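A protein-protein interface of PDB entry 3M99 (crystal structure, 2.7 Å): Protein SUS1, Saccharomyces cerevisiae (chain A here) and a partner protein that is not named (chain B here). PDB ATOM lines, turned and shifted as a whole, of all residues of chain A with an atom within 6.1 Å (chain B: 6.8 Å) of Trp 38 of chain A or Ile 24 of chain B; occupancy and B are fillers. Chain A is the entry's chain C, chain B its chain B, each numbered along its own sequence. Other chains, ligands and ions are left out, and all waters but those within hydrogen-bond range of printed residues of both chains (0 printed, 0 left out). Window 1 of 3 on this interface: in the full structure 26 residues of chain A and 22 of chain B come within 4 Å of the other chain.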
ATOM      1  N   ARG A  32      17.390  29.380  15.432  1.00  0.00           N
ATOM      2  CA  ARG A  32      17.484  28.880  14.068  1.00  0.00           C
ATOM      3  C   ARG A  32      18.258  27.565  13.978  1.00  0.00           C
ATOM      4  O   ARG A  32      17.930  26.688  13.175  1.00  0.00           O
ATOM      5  CB  ARG A  32      18.136  29.922  13.168  1.00  0.00           C
ATOM      6  CG  ARG A  32      17.207  31.032  12.747  1.00  0.00           C
ATOM      7  CD  ARG A  32      17.882  31.948  11.751  1.00  0.00           C
ATOM      8  NE  ARG A  32      16.929  32.510  10.803  1.00  0.00           N
ATOM      9  CZ  ARG A  32      16.132  33.538  11.069  1.00  0.00           C
ATOM     10  NH1 ARG A  32      16.170  34.116  12.264  1.00  0.00           N
ATOM     11  NH2 ARG A  32      15.295  33.983  10.144  1.00  0.00           N
ATOM     12  N   LEU A  33      19.294  27.432  14.798  1.00  0.00           N
ATOM     13  CA  LEU A  33      20.098  26.219  14.798  1.00  0.00           C
ATOM     14  C   LEU A  33      19.386  25.062  15.489  1.00  0.00           C
ATOM     15  O   LEU A  33      19.530  23.912  15.088  1.00  0.00           O
ATOM     16  CB  LEU A  33      21.452  26.473  15.458  1.00  0.00           C
ATOM     17  CG  LEU A  33      22.465  27.220  14.595  1.00  0.00           C
ATOM     18  CD1 LEU A  33      23.714  27.570  15.403  1.00  0.00           C
ATOM     19  CD2 LEU A  33      22.812  26.390  13.364  1.00  0.00           C
ATOM     20  N   LEU A  34      18.619  25.372  16.527  1.00  0.00           N
ATOM     21  CA  LEU A  34      17.929  24.340  17.284  1.00  0.00           C
ATOM     22  C   LEU A  34      16.784  23.742  16.484  1.00  0.00           C
ATOM     23  O   LEU A  34      16.571  22.532  16.522  1.00  0.00           O
ATOM     24  CB  LEU A  34      17.411  24.877  18.617  1.00  0.00           C
ATOM     25  CG  LEU A  34      16.587  23.845  19.387  1.00  0.00           C
ATOM     26  CD1 LEU A  34      17.388  22.576  19.598  1.00  0.00           C
ATOM     27  CD2 LEU A  34      16.114  24.397  20.714  1.00  0.00           C
ATOM     28  N   GLN A  35      16.058  24.590  15.759  1.00  0.00           N
ATOM     29  CA  GLN A  35      14.902  24.152  14.977  1.00  0.00           C
ATOM     30  C   GLN A  35      15.280  23.333  13.741  1.00  0.00           C
ATOM     31  O   GLN A  35      14.567  22.399  13.376  1.00  0.00           O
ATOM     32  CB  GLN A  35      14.044  25.348  14.564  1.00  0.00           C
ATOM     33  CG  GLN A  35      13.474  26.135  15.735  1.00  0.00           C
ATOM     34  CD  GLN A  35      12.018  26.518  15.529  1.00  0.00           C
ATOM     35  OE1 GLN A  35      11.260  25.798  14.868  1.00  0.00           O
ATOM     36  NE2 GLN A  35      11.613  27.650  16.105  1.00  0.00           N
ATOM     37  N   GLU A  36      16.399  23.686  13.109  1.00  0.00           N
ATOM     38  CA  GLU A  36      16.870  23.029  11.886  1.00  0.00           C
ATOM     39  C   GLU A  36      17.506  21.657  12.120  1.00  0.00           C
ATOM     40  O   GLU A  36      18.128  21.089  11.212  1.00  0.00           O
ATOM     41  CB  GLU A  36      17.908  23.900  11.179  1.00  0.00           C
ATOM     42  CG  GLU A  36      17.402  25.205  10.600  1.00  0.00           C
ATOM     43  CD  GLU A  36      18.522  25.980   9.917  1.00  0.00           C
ATOM     44  OE1 GLU A  36      19.681  25.878  10.384  1.00  0.00           O
ATOM     45  OE2 GLU A  36      18.248  26.681   8.916  1.00  0.00           O
ATOM     46  N   GLY A  37      17.376  21.140  13.337  1.00  0.00           N
ATOM     47  CA  GLY A  37      17.962  19.855  13.689  1.00  0.00           C
ATOM     48  C   GLY A  37      19.475  19.847  13.604  1.00  0.00           C
ATOM     49  O   GLY A  37      20.104  18.790  13.493  1.00  0.00           O
ATOM     50  N   TRP A  38      20.050  21.043  13.644  1.00  0.00           N
ATOM     51  CA  TRP A  38      21.490  21.214  13.607  1.00  0.00           C
ATOM     52  C   TRP A  38      22.105  20.767  14.926  1.00  0.00           C
ATOM     53  O   TRP A  38      22.941  19.874  14.940  1.00  0.00           O
ATOM     54  CB  TRP A  38      21.845  22.672  13.311  1.00  0.00           C
ATOM     55  CG  TRP A  38      23.306  22.913  13.173  1.00  0.00           C
ATOM     56  CD1 TRP A  38      24.071  22.704  12.060  1.00  0.00           C
ATOM     57  CD2 TRP A  38      24.192  23.412  14.181  1.00  0.00           C
ATOM     58  NE1 TRP A  38      25.379  23.042  12.316  1.00  0.00           N
ATOM     59  CE2 TRP A  38      25.479  23.479  13.611  1.00  0.00           C
ATOM     60  CE3 TRP A  38      24.024  23.807  15.513  1.00  0.00           C
ATOM     61  CZ2 TRP A  38      26.589  23.927  14.323  1.00  0.00           C
ATOM     62  CZ3 TRP A  38      25.134  24.251  16.220  1.00  0.00           C
ATOM     63  CH2 TRP A  38      26.396  24.307  15.622  1.00  0.00           C
ATOM     64  N   VAL A  39      21.682  21.382  16.029  1.00  0.00           N
ATOM     65  CA  VAL A  39      22.213  21.039  17.345  1.00  0.00           C
ATOM     66  C   VAL A  39      22.165  19.538  17.548  1.00  0.00           C
ATOM     67  O   VAL A  39      23.157  18.929  17.945  1.00  0.00           O
ATOM     68  CB  VAL A  39      21.438  21.724  18.491  1.00  0.00           C
ATOM     69  CG1 VAL A  39      21.966  21.257  19.839  1.00  0.00           C
ATOM     70  CG2 VAL A  39      21.528  23.232  18.373  1.00  0.00           C
ATOM     71  N   ASP A  40      21.006  18.951  17.262  1.00  0.00           N
ATOM     72  CA  ASP A  40      20.802  17.509  17.369  1.00  0.00           C
ATOM     73  C   ASP A  40      21.760  16.732  16.469  1.00  0.00           C
ATOM     74  O   ASP A  40      22.288  15.690  16.865  1.00  0.00           O
ATOM     75  CB  ASP A  40      19.368  17.140  16.989  1.00  0.00           C
ATOM     76  CG  ASP A  40      18.325  17.850  17.841  1.00  0.00           C
ATOM     77  OD1 ASP A  40      18.537  19.032  18.205  1.00  0.00           O
ATOM     78  OD2 ASP A  40      17.274  17.224  18.129  1.00  0.00           O
ATOM     79  N   LYS A  41      21.970  17.239  15.256  1.00  0.00           N
ATOM     80  CA  LYS A  41      22.796  16.554  14.261  1.00  0.00           C
ATOM     81  C   LYS A  41      24.288  16.674  14.585  1.00  0.00           C
ATOM     82  O   LYS A  41      25.078  15.782  14.271  1.00  0.00           O
ATOM     83  CB  LYS A  41      22.504  17.088  12.850  1.00  0.00           C
ATOM     84  CG  LYS A  41      22.479  16.003  11.770  1.00  0.00           C
ATOM     85  CD  LYS A  41      22.385  16.580  10.355  1.00  0.00           C
ATOM     86  CE  LYS A  41      22.500  15.469   9.302  1.00  0.00           C
ATOM     87  NZ  LYS A  41      22.616  15.977   7.899  1.00  0.00           N
ATOM     88  N   VAL A  42      24.657  17.787  15.212  1.00  0.00           N
ATOM     89  CA  VAL A  42      26.024  18.016  15.649  1.00  0.00           C
ATOM     90  C   VAL A  42      26.300  17.163  16.880  1.00  0.00           C
ATOM     91  O   VAL A  42      27.399  16.640  17.049  1.00  0.00           O
ATOM     92  CB  VAL A  42      26.263  19.509  15.966  1.00  0.00           C
ATOM     93  CG1 VAL A  42      27.561  19.703  16.719  1.00  0.00           C
ATOM     94  CG2 VAL A  42      26.259  20.332  14.688  1.00  0.00           C
ATOM     95  N   LYS A  43      25.295  17.017  17.737  1.00  0.00           N
ATOM     96  CA  LYS A  43      25.418  16.156  18.907  1.00  0.00           C
ATOM     97  C   LYS A  43      25.590  14.684  18.493  1.00  0.00           C
ATOM     98  O   LYS A  43      26.153  13.884  19.241  1.00  0.00           O
ATOM     99  CB  LYS A  43      24.214  16.333  19.855  1.00  0.00           C
ATOM    100  CG  LYS A  43      24.112  17.726  20.496  1.00  0.00           C
ATOM    101  CD  LYS A  43      22.965  17.854  21.509  1.00  0.00           C
ATOM    102  CE  LYS A  43      23.144  16.912  22.699  1.00  0.00           C
ATOM    103  NZ  LYS A  43      22.052  17.000  23.720  1.00  0.00           N
ATOM    104  N   THR A  46      29.214  14.095  16.791  1.00  0.00           N
ATOM    105  CA  THR A  46      30.219  13.977  17.836  1.00  0.00           C
ATOM    106  C   THR A  46      30.337  12.526  18.306  1.00  0.00           C
ATOM    107  O   THR A  46      31.442  12.017  18.485  1.00  0.00           O
ATOM    108  CB  THR A  46      29.939  14.951  19.016  1.00  0.00           C
ATOM    109  OG1 THR A  46      30.159  16.298  18.583  1.00  0.00           O
ATOM    110  CG2 THR A  46      30.850  14.669  20.192  1.00  0.00           C
ATOM    111  N   PHE A  58      38.625  15.680  24.295  1.00  0.00           N
ATOM    112  CA  PHE A  58      37.968  16.868  23.770  1.00  0.00           C
ATOM    113  C   PHE A  58      38.671  17.490  22.560  1.00  0.00           C
ATOM    114  O   PHE A  58      38.033  17.728  21.531  1.00  0.00           O
ATOM    115  CB  PHE A  58      37.780  17.920  24.860  1.00  0.00           C
ATOM    116  CG  PHE A  58      37.163  19.185  24.359  1.00  0.00           C
ATOM    117  CD1 PHE A  58      35.790  19.326  24.315  1.00  0.00           C
ATOM    118  CD2 PHE A  58      37.954  20.224  23.911  1.00  0.00           C
ATOM    119  CE1 PHE A  58      35.220  20.484  23.847  1.00  0.00           C
ATOM    120  CE2 PHE A  58      37.389  21.384  23.441  1.00  0.00           C
ATOM    121  CZ  PHE A  58      36.019  21.514  23.410  1.00  0.00           C
ATOM    122  N   LEU A  62      37.188  17.427  18.879  1.00  0.00           N
ATOM    123  CA  LEU A  62      36.809  18.758  18.414  1.00  0.00           C
ATOM    124  C   LEU A  62      37.408  19.126  17.059  1.00  0.00           C
ATOM    125  O   LEU A  62      36.780  19.836  16.276  1.00  0.00           O
ATOM    126  CB  LEU A  62      37.191  19.826  19.439  1.00  0.00           C
ATOM    127  CG  LEU A  62      37.132  21.270  18.924  1.00  0.00           C
ATOM    128  CD1 LEU A  62      35.704  21.697  18.605  1.00  0.00           C
ATOM    129  CD2 LEU A  62      37.750  22.220  19.924  1.00  0.00           C
ATOM    130  N   VAL A  65      35.134  17.440  14.392  1.00  0.00           N
ATOM    131  CA  VAL A  65      33.739  17.864  14.444  1.00  0.00           C
ATOM    132  C   VAL A  65      33.535  19.328  14.067  1.00  0.00           C
ATOM    133  O   VAL A  65      32.604  19.651  13.334  1.00  0.00           O
ATOM    134  CB  VAL A  65      33.114  17.641  15.835  1.00  0.00           C
ATOM    135  CG1 VAL A  65      31.718  18.264  15.891  1.00  0.00           C
ATOM    136  CG2 VAL A  65      33.064  16.156  16.171  1.00  0.00           C
ATOM    137  N   GLU A  66      34.391  20.211  14.575  1.00  0.00           N
ATOM    138  CA  GLU A  66      34.195  21.648  14.386  1.00  0.00           C
ATOM    139  C   GLU A  66      34.137  22.094  12.917  1.00  0.00           C
ATOM    140  O   GLU A  66      33.237  22.845  12.538  1.00  0.00           O
ATOM    141  CB  GLU A  66      35.235  22.469  15.169  1.00  0.00           C
ATOM    142  CG  GLU A  66      35.183  23.978  14.883  1.00  0.00           C
ATOM    143  CD  GLU A  66      36.127  24.791  15.760  1.00  0.00           C
ATOM    144  OE1 GLU A  66      35.991  24.712  16.999  1.00  0.00           O
ATOM    145  OE2 GLU A  66      36.991  25.520  15.214  1.00  0.00           O
ATOM    146  N   LYS A  68      33.470  20.255  10.165  1.00  0.00           N
ATOM    147  CA  LYS A  68      32.256  19.662   9.603  1.00  0.00           C
ATOM    148  C   LYS A  68      31.029  20.388  10.111  1.00  0.00           C
ATOM    149  O   LYS A  68      30.196  20.867   9.337  1.00  0.00           O
ATOM    150  CB  LYS A  68      32.133  18.194  10.011  1.00  0.00           C
ATOM    151  CG  LYS A  68      33.033  17.252   9.255  1.00  0.00           C
ATOM    152  CD  LYS A  68      32.781  15.814   9.689  1.00  0.00           C
ATOM    153  CE  LYS A  68      33.800  14.857   9.080  1.00  0.00           C
ATOM    154  NZ  LYS A  68      33.671  13.463   9.603  1.00  0.00           N
ATOM    155  N   ALA A  69      30.920  20.437  11.433  1.00  0.00           N
ATOM    156  CA  ALA A  69      29.809  21.094  12.094  1.00  0.00           C
ATOM    157  C   ALA A  69      29.723  22.555  11.671  1.00  0.00           C
ATOM    158  O   ALA A  69      28.707  23.212  11.885  1.00  0.00           O
ATOM    159  CB  ALA A  69      29.955  20.977  13.602  1.00  0.00           C
ATOM    160  N   LEU A  70      30.788  23.057  11.056  1.00  0.00           N
ATOM    161  CA  LEU A  70      30.829  24.452  10.637  1.00  0.00           C
ATOM    162  C   LEU A  70      30.211  24.605   9.247  1.00  0.00           C
ATOM    163  O   LEU A  70      29.603  25.631   8.932  1.00  0.00           O
ATOM    164  CB  LEU A  70      32.269  24.978  10.681  1.00  0.00           C
ATOM    165  CG  LEU A  70      32.461  26.487  10.858  1.00  0.00           C
ATOM    166  CD1 LEU A  70      31.249  27.115  11.520  1.00  0.00           C
ATOM    167  CD2 LEU A  70      33.732  26.786  11.652  1.00  0.00           C
ATOM    168  N   GLU A  71      30.360  23.567   8.431  1.00  0.00           N
ATOM    169  CA  GLU A  71      29.724  23.512   7.123  1.00  0.00           C
ATOM    170  C   GLU A  71      28.253  23.123   7.255  1.00  0.00           C
ATOM    171  O   GLU A  71      27.435  23.472   6.408  1.00  0.00           O
ATOM    172  CB  GLU A  71      30.450  22.504   6.230  1.00  0.00           C
ATOM    173  CG  GLU A  71      31.760  23.019   5.648  1.00  0.00           C
ATOM    174  CD  GLU A  71      31.549  24.049   4.543  1.00  0.00           C
ATOM    175  OE1 GLU A  71      32.546  24.660   4.101  1.00  0.00           O
ATOM    176  OE2 GLU A  71      30.389  24.241   4.113  1.00  0.00           O
ATOM    177  N   MET A  72      27.926  22.415   8.333  1.00  0.00           N
ATOM    178  CA  MET A  72      26.596  21.837   8.516  1.00  0.00           C
ATOM    179  C   MET A  72      25.474  22.874   8.685  1.00  0.00           C
ATOM    180  O   MET A  72      24.288  22.538   8.609  1.00  0.00           O
ATOM    181  CB  MET A  72      26.615  20.873   9.702  1.00  0.00           C
ATOM    182  CG  MET A  72      25.751  19.645   9.519  1.00  0.00           C
ATOM    183  SD  MET A  72      26.391  18.249  10.465  1.00  0.00           S
ATOM    184  CE  MET A  72      27.797  17.785   9.456  1.00  0.00           C
ATOM    185  N   VAL A  73      25.851  24.128   8.920  1.00  0.00           N
ATOM    186  CA  VAL A  73      24.872  25.202   9.030  1.00  0.00           C
ATOM    187  C   VAL A  73      24.232  25.489   7.679  1.00  0.00           C
ATOM    188  O   VAL A  73      24.914  25.581   6.656  1.00  0.00           O
ATOM    189  CB  VAL A  73      25.467  26.504   9.635  1.00  0.00           C
ATOM    190  CG1 VAL A  73      26.204  26.188  10.918  1.00  0.00           C
ATOM    191  CG2 VAL A  73      26.376  27.223   8.634  1.00  0.00           C
ATOM    192  N   SER A  74      22.908  25.600   7.673  1.00  0.00           N
ATOM    193  CA  SER A  74      22.204  26.002   6.459  1.00  0.00           C
ATOM    194  C   SER A  74      22.739  27.334   5.943  1.00  0.00           C
ATOM    195  O   SER A  74      22.906  28.286   6.710  1.00  0.00           O
ATOM    196  CB  SER A  74      20.703  26.145   6.709  1.00  0.00           C
ATOM    197  OG  SER A  74      20.437  27.307   7.478  1.00  0.00           O
ATOM    198  N   LEU B  19      30.524  33.108  17.697  1.00  0.00           N
ATOM    199  CA  LEU B  19      29.295  32.518  18.221  1.00  0.00           C
ATOM    200  C   LEU B  19      29.191  31.047  17.827  1.00  0.00           C
ATOM    201  O   LEU B  19      28.806  30.206  18.635  1.00  0.00           O
ATOM    202  CB  LEU B  19      28.072  33.285  17.706  1.00  0.00           C
ATOM    203  CG  LEU B  19      27.889  34.727  18.185  1.00  0.00           C
ATOM    204  CD1 LEU B  19      26.929  35.489  17.284  1.00  0.00           C
ATOM    205  CD2 LEU B  19      27.420  34.760  19.633  1.00  0.00           C
ATOM    206  N   LEU B  20      29.547  30.747  16.582  1.00  0.00           N
ATOM    207  CA  LEU B  20      29.470  29.388  16.068  1.00  0.00           C
ATOM    208  C   LEU B  20      30.416  28.452  16.801  1.00  0.00           C
ATOM    209  O   LEU B  20      30.043  27.336  17.167  1.00  0.00           O
ATOM    210  CB  LEU B  20      29.762  29.360  14.567  1.00  0.00           C
ATOM    211  CG  LEU B  20      28.545  29.577  13.662  1.00  0.00           C
ATOM    212  CD1 LEU B  20      28.932  29.619  12.188  1.00  0.00           C
ATOM    213  CD2 LEU B  20      27.513  28.494  13.913  1.00  0.00           C
ATOM    214  N   THR B  21      31.642  28.911  17.021  1.00  0.00           N
ATOM    215  CA  THR B  21      32.670  28.068  17.620  1.00  0.00           C
ATOM    216  C   THR B  21      32.393  27.804  19.095  1.00  0.00           C
ATOM    217  O   THR B  21      32.481  26.665  19.550  1.00  0.00           O
ATOM    218  CB  THR B  21      34.086  28.654  17.424  1.00  0.00           C
ATOM    219  OG1 THR B  21      34.069  30.065  17.678  1.00  0.00           O
ATOM    220  CG2 THR B  21      34.569  28.410  15.999  1.00  0.00           C
ATOM    221  N   THR B  22      32.050  28.854  19.834  1.00  0.00           N
ATOM    222  CA  THR B  22      31.693  28.702  21.237  1.00  0.00           C
ATOM    223  C   THR B  22      30.585  27.667  21.389  1.00  0.00           C
ATOM    224  O   THR B  22      30.521  26.942  22.381  1.00  0.00           O
ATOM    225  CB  THR B  22      31.171  30.014  21.826  1.00  0.00           C
ATOM    226  OG1 THR B  22      31.939  31.117  21.328  1.00  0.00           O
ATOM    227  CG2 THR B  22      31.240  29.971  23.342  1.00  0.00           C
ATOM    228  N   LEU B  23      29.715  27.612  20.387  1.00  0.00           N
ATOM    229  CA  LEU B  23      28.533  26.768  20.423  1.00  0.00           C
ATOM    230  C   LEU B  23      28.904  25.342  20.044  1.00  0.00           C
ATOM    231  O   LEU B  23      28.395  24.378  20.625  1.00  0.00           O
ATOM    232  CB  LEU B  23      27.476  27.319  19.464  1.00  0.00           C
ATOM    233  CG  LEU B  23      25.999  27.123  19.797  1.00  0.00           C
ATOM    234  CD1 LEU B  23      25.151  27.864  18.779  1.00  0.00           C
ATOM    235  CD2 LEU B  23      25.616  25.649  19.842  1.00  0.00           C
ATOM    236  N   ILE B  24      29.795  25.212  19.066  1.00  0.00           N
ATOM    237  CA  ILE B  24      30.298  23.899  18.687  1.00  0.00           C
ATOM    238  C   ILE B  24      31.086  23.291  19.842  1.00  0.00           C
ATOM    239  O   ILE B  24      30.921  22.115  20.169  1.00  0.00           O
ATOM    240  CB  ILE B  24      31.217  23.964  17.467  1.00  0.00           C
ATOM    241  CG1 ILE B  24      30.531  24.674  16.305  1.00  0.00           C
ATOM    242  CG2 ILE B  24      31.597  22.568  17.050  1.00  0.00           C
ATOM    243  CD1 ILE B  24      29.670  23.773  15.488  1.00  0.00           C
ATOM    244  N   GLN B  25      31.936  24.104  20.463  1.00  0.00           N
ATOM    245  CA  GLN B  25      32.791  23.650  21.552  1.00  0.00           C
ATOM    246  C   GLN B  25      31.993  23.274  22.799  1.00  0.00           C
ATOM    247  O   GLN B  25      32.366  22.357  23.526  1.00  0.00           O
ATOM    248  CB  GLN B  25      33.836  24.715  21.893  1.00  0.00           C
ATOM    249  CG  GLN B  25      34.776  25.079  20.750  1.00  0.00           C
ATOM    250  CD  GLN B  25      35.830  26.083  21.178  1.00  0.00           C
ATOM    251  OE1 GLN B  25      36.219  26.127  22.346  1.00  0.00           O
ATOM    252  NE2 GLN B  25      36.294  26.897  20.235  1.00  0.00           N
ATOM    253  N   ASP B  26      30.899  23.989  23.048  1.00  0.00           N
ATOM    254  CA  ASP B  26      29.988  23.648  24.144  1.00  0.00           C
ATOM    255  C   ASP B  26      29.258  22.322  23.870  1.00  0.00           C
ATOM    256  O   ASP B  26      29.227  21.438  24.729  1.00  0.00           O
ATOM    257  CB  ASP B  26      28.994  24.790  24.402  1.00  0.00           C
ATOM    258  CG  ASP B  26      27.960  24.447  25.471  1.00  0.00           C
ATOM    259  OD1 ASP B  26      28.178  23.474  26.228  1.00  0.00           O
ATOM    260  OD2 ASP B  26      26.926  25.154  25.558  1.00  0.00           O
ATOM    261  N   ILE B  27      28.681  22.177  22.680  1.00  0.00           N
ATOM    262  CA  ILE B  27      27.991  20.938  22.332  1.00  0.00           C
ATOM    263  C   ILE B  27      28.888  19.716  22.549  1.00  0.00           C
ATOM    264  O   ILE B  27      28.495  18.766  23.231  1.00  0.00           O
ATOM    265  CB  ILE B  27      27.504  20.922  20.861  1.00  0.00           C
ATOM    266  CG1 ILE B  27      26.581  22.106  20.555  1.00  0.00           C
ATOM    267  CG2 ILE B  27      26.819  19.610  20.543  1.00  0.00           C
ATOM    268  CD1 ILE B  27      25.368  22.198  21.428  1.00  0.00           C
ATOM    269  N   VAL B  28      30.089  19.751  21.963  1.00  0.00           N
ATOM    270  CA  VAL B  28      31.042  18.637  22.013  1.00  0.00           C
ATOM    271  C   VAL B  28      31.537  18.372  23.429  1.00  0.00           C
ATOM    272  O   VAL B  28      31.654  17.224  23.859  1.00  0.00           O
ATOM    273  CB  VAL B  28      32.262  18.911  21.111  1.00  0.00           C
ATOM    274  CG1 VAL B  28      33.255  17.757  21.182  1.00  0.00           C
ATOM    275  CG2 VAL B  28      31.819  19.161  19.673  1.00  0.00           C
ATOM    276  N   ALA B  29      31.822  19.452  24.147  1.00  0.00           N
ATOM    277  CA  ALA B  29      32.321  19.374  25.514  1.00  0.00           C
ATOM    278  C   ALA B  29      31.428  18.543  26.425  1.00  0.00           C
ATOM    279  O   ALA B  29      31.908  17.913  27.367  1.00  0.00           O
ATOM    280  CB  ALA B  29      32.480  20.765  26.086  1.00  0.00           C
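The backbone carbonyl oxygen (O) of Leu 33 of chain A lies close to the backbone NH (N) of Trp 38 of chain A, at 3.3 Å. O of Leu 33 of chain A lies within hydrogen-bond range of N of Val 39 of chain A (3.5 Å). NE1 of Trp 38 of chain A lies close to O of Ala 69 of chain A. The backbone carbonyl oxygen (O) of Val 42 of chain A is in hydrogen-bond range of the side-chain hydroxyl (OG1) of Thr 46 of chain A.
Among the printed residues, pairs that only touch across the chains: Trp 38 of chain A with Ile 24 of chain B (3.3 Å), Lys 43 of chain A with Ile 27 of chain B (3.3 Å), Ala 69 of chain A with Ile 24 of chain B (3.4 Å), Phe 58 of chain A with Gln 25 of chain B (3.4 Å), Leu 70 of chain A with Leu 20 of chain B (3.5 Å), Thr 46 of chain A with Val 28 of chain B (3.5 Å), Phe 58 of chain A with Ala 29 of chain B (3.5 Å), Leu 33 of chain A with Leu 23 of chain B (3.7 Å), Glu 66 of chain A with Ile 24 of chain B (3.8 Å), Glu 66 of chain A with Thr 21 of chain B (3.9 Å), Val 39 of chain A with Ile 27 of chain B (3.9 Å), Val 65 of chain A with Val 28 of chain B (3.9 Å), Val 42 of chain A with Ile 27 of chain B (3.9 Å), Trp 38 of chain A with Leu 23 of chain B (3.9 Å) and Glu 66 of chain A with Gln 25 of chain B (3.9 Å).
Glu 36 of chain A touches none of the printed residues of chain B. Trp 38 of chain A touches just these residues of chain B: Leu 23 and Ile 24. Of the printed residues of chain B, Glu 66 of chain A touches Thr 21 (3.9 Å), Ile 24 (3.8 Å) and Gln 25 (3.9 Å). Met 72 of chain A touches none of the printed residues of chain B. Of the printed residues of chain A, Leu 20 of chain B touches Leu 70 (3.5 Å). Ile 24 of chain B touches three residues of chain A. The nearest printed residue of chain B that does not touch Val 42 of chain A is Ile 24 of chain B (4.7 Å).
Of the 11 printed residues of chain B, 8 touch a printed residue of chain A. Printed residues of chain B that touch a printed residue of chain A: Leu 20, Thr 21, Leu 23, Ile 24, Gln 25, Ile 27, Val 28 and Ala 29. Of the 24 printed residues of chain A, 11 touch a printed residue of chain B.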
